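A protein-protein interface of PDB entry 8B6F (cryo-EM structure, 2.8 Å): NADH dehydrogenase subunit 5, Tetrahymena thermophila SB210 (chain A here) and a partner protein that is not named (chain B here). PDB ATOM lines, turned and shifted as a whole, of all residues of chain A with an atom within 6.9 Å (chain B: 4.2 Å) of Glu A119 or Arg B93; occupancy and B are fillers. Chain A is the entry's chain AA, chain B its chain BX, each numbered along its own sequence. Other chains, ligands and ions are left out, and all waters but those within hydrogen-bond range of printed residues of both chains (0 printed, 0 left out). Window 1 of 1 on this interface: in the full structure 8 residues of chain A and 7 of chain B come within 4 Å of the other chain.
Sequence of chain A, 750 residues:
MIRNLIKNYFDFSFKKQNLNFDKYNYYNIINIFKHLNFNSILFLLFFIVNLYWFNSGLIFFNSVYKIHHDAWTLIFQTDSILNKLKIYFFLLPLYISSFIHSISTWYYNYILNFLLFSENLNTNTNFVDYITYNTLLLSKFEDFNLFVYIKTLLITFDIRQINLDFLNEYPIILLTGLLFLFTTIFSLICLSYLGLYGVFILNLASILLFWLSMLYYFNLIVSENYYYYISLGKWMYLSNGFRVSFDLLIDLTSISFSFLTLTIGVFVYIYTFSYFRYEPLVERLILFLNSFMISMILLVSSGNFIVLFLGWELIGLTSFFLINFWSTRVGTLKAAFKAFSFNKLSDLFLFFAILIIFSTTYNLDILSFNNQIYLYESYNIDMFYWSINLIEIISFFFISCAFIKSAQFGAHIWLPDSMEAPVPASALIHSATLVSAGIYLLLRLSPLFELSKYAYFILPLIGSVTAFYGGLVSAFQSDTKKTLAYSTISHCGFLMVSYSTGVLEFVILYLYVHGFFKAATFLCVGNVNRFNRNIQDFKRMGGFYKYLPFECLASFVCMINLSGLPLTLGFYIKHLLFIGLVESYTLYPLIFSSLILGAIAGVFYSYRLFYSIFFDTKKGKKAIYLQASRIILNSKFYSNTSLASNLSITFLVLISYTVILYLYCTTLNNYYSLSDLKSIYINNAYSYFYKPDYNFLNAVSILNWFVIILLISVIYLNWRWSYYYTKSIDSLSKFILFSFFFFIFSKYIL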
ATOM      1  N   LEU A 112      31.257  -5.598  25.566  1.00  0.00           N
ATOM      2  CA  LEU A 112      29.881  -5.331  25.165  1.00  0.00           C
ATOM      3  C   LEU A 112      29.812  -4.855  23.722  1.00  0.00           C
ATOM      4  O   LEU A 112      28.943  -5.291  22.958  1.00  0.00           O
ATOM      5  CB  LEU A 112      29.247  -4.296  26.092  1.00  0.00           C
ATOM      6  CG  LEU A 112      29.035  -4.686  27.557  1.00  0.00           C
ATOM      7  CD1 LEU A 112      28.046  -3.728  28.198  1.00  0.00           C
ATOM      8  CD2 LEU A 112      28.598  -6.127  27.710  1.00  0.00           C
ATOM      9  N   ASN A 113      30.711  -3.954  23.328  1.00  0.00           N
ATOM     10  CA  ASN A 113      30.723  -3.498  21.944  1.00  0.00           C
ATOM     11  C   ASN A 113      31.020  -4.652  20.999  1.00  0.00           C
ATOM     12  O   ASN A 113      30.398  -4.775  19.937  1.00  0.00           O
ATOM     13  CB  ASN A 113      31.751  -2.383  21.767  1.00  0.00           C
ATOM     14  CG  ASN A 113      31.422  -1.156  22.585  1.00  0.00           C
ATOM     15  OD1 ASN A 113      30.577  -1.199  23.478  1.00  0.00           O
ATOM     16  ND2 ASN A 113      32.095  -0.053  22.289  1.00  0.00           N
ATOM     17  N   LEU A 116      27.785  -6.929  20.835  1.00  0.00           N
ATOM     18  CA  LEU A 116      26.524  -6.347  20.398  1.00  0.00           C
ATOM     19  C   LEU A 116      26.655  -5.444  19.180  1.00  0.00           C
ATOM     20  O   LEU A 116      25.643  -4.905  18.722  1.00  0.00           O
ATOM     21  CB  LEU A 116      25.889  -5.563  21.554  1.00  0.00           C
ATOM     22  CG  LEU A 116      25.065  -6.372  22.563  1.00  0.00           C
ATOM     23  CD1 LEU A 116      25.703  -7.714  22.884  1.00  0.00           C
ATOM     24  CD2 LEU A 116      24.875  -5.574  23.840  1.00  0.00           C
ATOM     25  N   PHE A 117      27.859  -5.268  18.637  1.00  0.00           N
ATOM     26  CA  PHE A 117      28.057  -4.432  17.453  1.00  0.00           C
ATOM     27  C   PHE A 117      27.461  -3.044  17.662  1.00  0.00           C
ATOM     28  O   PHE A 117      26.886  -2.450  16.748  1.00  0.00           O
ATOM     29  CB  PHE A 117      27.441  -5.086  16.214  1.00  0.00           C
ATOM     30  CG  PHE A 117      28.125  -6.347  15.778  1.00  0.00           C
ATOM     31  CD1 PHE A 117      28.054  -7.493  16.551  1.00  0.00           C
ATOM     32  CD2 PHE A 117      28.807  -6.398  14.575  1.00  0.00           C
ATOM     33  CE1 PHE A 117      28.671  -8.659  16.146  1.00  0.00           C
ATOM     34  CE2 PHE A 117      29.426  -7.560  14.163  1.00  0.00           C
ATOM     35  CZ  PHE A 117      29.357  -8.693  14.951  1.00  0.00           C
ATOM     36  N   SER A 118      27.599  -2.514  18.874  1.00  0.00           N
ATOM     37  CA  SER A 118      26.848  -1.340  19.295  1.00  0.00           C
ATOM     38  C   SER A 118      27.778  -0.231  19.762  1.00  0.00           C
ATOM     39  O   SER A 118      28.647  -0.457  20.610  1.00  0.00           O
ATOM     40  CB  SER A 118      25.868  -1.698  20.416  1.00  0.00           C
ATOM     41  OG  SER A 118      26.552  -2.196  21.552  1.00  0.00           O
ATOM     42  N   GLU A 119      27.580   0.964  19.204  1.00  0.00           N
ATOM     43  CA  GLU A 119      28.135   2.212  19.720  1.00  0.00           C
ATOM     44  C   GLU A 119      29.602   2.112  20.123  1.00  0.00           C
ATOM     45  O   GLU A 119      30.320   1.207  19.688  1.00  0.00           O
ATOM     46  CB  GLU A 119      27.299   2.685  20.918  1.00  0.00           C
ATOM     47  CG  GLU A 119      27.435   1.822  22.172  1.00  0.00           C
ATOM     48  CD  GLU A 119      26.660   2.381  23.347  1.00  0.00           C
ATOM     49  OE1 GLU A 119      25.913   3.362  23.153  1.00  0.00           O
ATOM     50  OE2 GLU A 119      26.799   1.841  24.465  1.00  0.00           O
ATOM     51  N   ASN A 120      30.051   3.060  20.941  1.00  0.00           N
ATOM     52  CA  ASN A 120      31.399   3.098  21.489  1.00  0.00           C
ATOM     53  C   ASN A 120      31.307   3.087  23.014  1.00  0.00           C
ATOM     54  O   ASN A 120      30.241   2.858  23.592  1.00  0.00           O
ATOM     55  CB  ASN A 120      32.149   4.331  20.980  1.00  0.00           C
ATOM     56  CG  ASN A 120      32.008   4.525  19.483  1.00  0.00           C
ATOM     57  OD1 ASN A 120      31.842   3.562  18.734  1.00  0.00           O
ATOM     58  ND2 ASN A 120      32.071   5.775  19.040  1.00  0.00           N
ATOM     59  N   LEU A 121      32.440   3.340  23.669  1.00  0.00           N
ATOM     60  CA  LEU A 121      32.481   3.451  25.127  1.00  0.00           C
ATOM     61  C   LEU A 121      31.902   4.809  25.526  1.00  0.00           C
ATOM     62  O   LEU A 121      32.596   5.715  25.988  1.00  0.00           O
ATOM     63  CB  LEU A 121      33.902   3.272  25.645  1.00  0.00           C
ATOM     64  CG  LEU A 121      34.624   1.953  25.335  1.00  0.00           C
ATOM     65  CD1 LEU A 121      35.165   1.900  23.907  1.00  0.00           C
ATOM     66  CD2 LEU A 121      35.744   1.719  26.334  1.00  0.00           C
ATOM     67  N   ASN A 122      30.590   4.934  25.322  1.00  0.00           N
ATOM     68  CA  ASN A 122      29.895   6.206  25.477  1.00  0.00           C
ATOM     69  C   ASN A 122      30.400   7.182  24.421  1.00  0.00           C
ATOM     70  O   ASN A 122      29.649   7.584  23.527  1.00  0.00           O
ATOM     71  CB  ASN A 122      30.087   6.774  26.886  1.00  0.00           C
ATOM     72  CG  ASN A 122      29.231   7.998  27.142  1.00  0.00           C
ATOM     73  OD1 ASN A 122      29.642   9.126  26.868  1.00  0.00           O
ATOM     74  ND2 ASN A 122      28.030   7.781  27.670  1.00  0.00           N
ATOM     75  N   THR A 123      31.669   7.561  24.519  1.00  0.00           N
ATOM     76  CA  THR A 123      32.354   8.372  23.523  1.00  0.00           C
ATOM     77  C   THR A 123      33.512   7.568  22.932  1.00  0.00           C
ATOM     78  O   THR A 123      33.749   6.416  23.299  1.00  0.00           O
ATOM     79  CB  THR A 123      32.846   9.684  24.139  1.00  0.00           C
ATOM     80  OG1 THR A 123      33.527   9.415  25.371  1.00  0.00           O
ATOM     81  CG2 THR A 123      31.678  10.622  24.401  1.00  0.00           C
ATOM     82  N   VAL B  89      22.599  -9.786  28.554  1.00  0.00           N
ATOM     83  CA  VAL B  89      23.088  -8.468  28.164  1.00  0.00           C
ATOM     84  C   VAL B  89      22.442  -8.027  26.859  1.00  0.00           C
ATOM     85  O   VAL B  89      22.141  -6.844  26.668  1.00  0.00           O
ATOM     86  CB  VAL B  89      24.623  -8.465  28.072  1.00  0.00           C
ATOM     87  CG1 VAL B  89      25.110  -9.387  26.965  1.00  0.00           C
ATOM     88  CG2 VAL B  89      25.120  -7.057  27.859  1.00  0.00           C
ATOM     89  N   ALA B  90      22.224  -8.967  25.939  1.00  0.00           N
ATOM     90  CA  ALA B  90      21.557  -8.631  24.687  1.00  0.00           C
ATOM     91  C   ALA B  90      20.132  -8.162  24.938  1.00  0.00           C
ATOM     92  O   ALA B  90      19.664  -7.213  24.298  1.00  0.00           O
ATOM     93  CB  ALA B  90      21.569  -9.837  23.746  1.00  0.00           C
ATOM     94  N   TYR B  91      19.422  -8.814  25.859  1.00  0.00           N
ATOM     95  CA  TYR B  91      18.078  -8.356  26.192  1.00  0.00           C
ATOM     96  C   TYR B  91      18.110  -6.977  26.835  1.00  0.00           C
ATOM     97  O   TYR B  91      17.246  -6.139  26.554  1.00  0.00           O
ATOM     98  CB  TYR B  91      17.378  -9.345  27.119  1.00  0.00           C
ATOM     99  CG  TYR B  91      16.003  -8.859  27.508  1.00  0.00           C
ATOM    100  CD1 TYR B  91      14.927  -9.010  26.648  1.00  0.00           C
ATOM    101  CD2 TYR B  91      15.790  -8.217  28.720  1.00  0.00           C
ATOM    102  CE1 TYR B  91      13.673  -8.553  26.987  1.00  0.00           C
ATOM    103  CE2 TYR B  91      14.537  -7.754  29.069  1.00  0.00           C
ATOM    104  CZ  TYR B  91      13.483  -7.926  28.198  1.00  0.00           C
ATOM    105  OH  TYR B  91      12.232  -7.470  28.534  1.00  0.00           O
ATOM    106  N   GLU B  92      19.091  -6.720  27.701  1.00  0.00           N
ATOM    107  CA  GLU B  92      19.221  -5.389  28.285  1.00  0.00           C
ATOM    108  C   GLU B  92      19.369  -4.337  27.194  1.00  0.00           C
ATOM    109  O   GLU B  92      18.680  -3.312  27.204  1.00  0.00           O
ATOM    110  CB  GLU B  92      20.418  -5.349  29.233  1.00  0.00           C
ATOM    111  CG  GLU B  92      20.265  -6.211  30.471  1.00  0.00           C
ATOM    112  CD  GLU B  92      19.264  -5.646  31.455  1.00  0.00           C
ATOM    113  OE1 GLU B  92      18.681  -4.580  31.170  1.00  0.00           O
ATOM    114  OE2 GLU B  92      19.060  -6.268  32.517  1.00  0.00           O
ATOM    115  N   ARG B  93      20.276  -4.574  26.248  1.00  0.00           N
ATOM    116  CA  ARG B  93      20.489  -3.614  25.171  1.00  0.00           C
ATOM    117  C   ARG B  93      19.241  -3.471  24.311  1.00  0.00           C
ATOM    118  O   ARG B  93      18.893  -2.366  23.883  1.00  0.00           O
ATOM    119  CB  ARG B  93      21.687  -4.036  24.323  1.00  0.00           C
ATOM    120  CG  ARG B  93      22.272  -2.919  23.477  1.00  0.00           C
ATOM    121  CD  ARG B  93      22.992  -1.893  24.335  1.00  0.00           C
ATOM    122  NE  ARG B  93      23.687  -0.900  23.526  1.00  0.00           N
ATOM    123  CZ  ARG B  93      23.141   0.219  23.067  1.00  0.00           C
ATOM    124  NH1 ARG B  93      21.877   0.525  23.315  1.00  0.00           N
ATOM    125  NH2 ARG B  93      23.883   1.054  22.346  1.00  0.00           N
ATOM    126  N   SER B  94      18.555  -4.584  24.045  1.00  0.00           N
ATOM    127  CA  SER B  94      17.340  -4.531  23.239  1.00  0.00           C
ATOM    128  C   SER B  94      16.257  -3.709  23.923  1.00  0.00           C
ATOM    129  O   SER B  94      15.571  -2.911  23.274  1.00  0.00           O
ATOM    130  CB  SER B  94      16.833  -5.945  22.956  1.00  0.00           C
ATOM    131  OG  SER B  94      17.772  -6.686  22.199  1.00  0.00           O
ATOM    132  N   TYR B  95      16.085  -3.889  25.234  1.00  0.00           N
ATOM    133  CA  TYR B  95      15.093  -3.101  25.957  1.00  0.00           C
ATOM    134  C   TYR B  95      15.445  -1.622  25.935  1.00  0.00           C
ATOM    135  O   TYR B  95      14.567  -0.770  25.762  1.00  0.00           O
ATOM    136  CB  TYR B  95      14.968  -3.597  27.395  1.00  0.00           C
ATOM    137  CG  TYR B  95      14.041  -2.751  28.233  1.00  0.00           C
ATOM    138  CD1 TYR B  95      12.665  -2.887  28.130  1.00  0.00           C
ATOM    139  CD2 TYR B  95      14.543  -1.814  29.125  1.00  0.00           C
ATOM    140  CE1 TYR B  95      11.814  -2.112  28.892  1.00  0.00           C
ATOM    141  CE2 TYR B  95      13.702  -1.036  29.890  1.00  0.00           C
ATOM    142  CZ  TYR B  95      12.339  -1.190  29.770  1.00  0.00           C
ATOM    143  OH  TYR B  95      11.494  -0.419  30.532  1.00  0.00           O
ATOM    144  N   ALA B  96      16.725  -1.292  26.103  1.00  0.00           N
ATOM    145  CA  ALA B  96      17.131   0.104  26.019  1.00  0.00           C
ATOM    146  C   ALA B  96      16.807   0.679  24.646  1.00  0.00           C
ATOM    147  O   ALA B  96      16.312   1.805  24.537  1.00  0.00           O
ATOM    148  CB  ALA B  96      18.622   0.235  26.322  1.00  0.00           C
ATOM    149  N   SER B  97      17.089  -0.078  23.585  1.00  0.00           N
ATOM    150  CA  SER B  97      16.796   0.397  22.237  1.00  0.00           C
ATOM    151  C   SER B  97      15.298   0.588  22.029  1.00  0.00           C
ATOM    152  O   SER B  97      14.871   1.572  21.413  1.00  0.00           O
ATOM    153  CB  SER B  97      17.356  -0.579  21.206  1.00  0.00           C
ATOM    154  OG  SER B  97      18.765  -0.667  21.309  1.00  0.00           O
ATOM    155  N   TYR B 102      20.059   5.046  25.639  1.00  0.00           N
ATOM    156  CA  TYR B 102      21.345   4.363  25.575  1.00  0.00           C
ATOM    157  C   TYR B 102      21.487   3.302  26.655  1.00  0.00           C
ATOM    158  O   TYR B 102      22.339   2.418  26.529  1.00  0.00           O
ATOM    159  CB  TYR B 102      22.488   5.372  25.694  1.00  0.00           C
ATOM    160  CG  TYR B 102      22.627   6.285  24.499  1.00  0.00           C
ATOM    161  CD1 TYR B 102      23.143   5.813  23.299  1.00  0.00           C
ATOM    162  CD2 TYR B 102      22.256   7.620  24.574  1.00  0.00           C
ATOM    163  CE1 TYR B 102      23.276   6.644  22.203  1.00  0.00           C
ATOM    164  CE2 TYR B 102      22.386   8.458  23.486  1.00  0.00           C
ATOM    165  CZ  TYR B 102      22.896   7.966  22.303  1.00  0.00           C
ATOM    166  OH  TYR B 102      23.028   8.796  21.216  1.00  0.00           O
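Among the printed residues, pairs that only touch across the chains: Leu A112 with Val B89, Leu A116 with Arg B93, Ser A118 with Arg B93 and Glu A119 with Tyr B102.
Of the printed residues of chain B, Leu A112 touches Val B89.
Of the printed residues of chain B, Leu A116 touches Arg B93.
Printed residues of chain B within 4 Å of Ser A118: Arg B93.
Of chain B, only Arg B93 and Tyr B102 come within 4 Å of Glu A119.
Of chain A, only Leu A116, Ser A118 and Glu A119 come within 4 Å of Arg B93.
Of the printed residues of chain A, Tyr B102 touches Glu A119.
The side-chain amide nitrogen (ND2) of Asn A113 lies within hydrogen-bond range of the backbone carbonyl oxygen (O) of Glu A119, at 3.4 Å.
O of Arg B93 is in hydrogen-bond range of OG of Ser B97, 3.1 Å away.
The guanidinium group (NH2) of Arg B93 is in salt-bridge range of the side-chain carboxylate (OE1) of Glu A119 (3.2 Å).
Of the 10 printed residues of chain A, 4 touch a printed residue of chain B.
Hydrophobic or aromatic side chains of chain A that line the printed part of chain B: Leu A112 and Leu A116.
Among the printed residues, Asp or Glu carboxylates within 4 Å of a Lys or Arg side-chain nitrogen of the other chain: Glu A119 with Arg B93 (3.2 Å).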
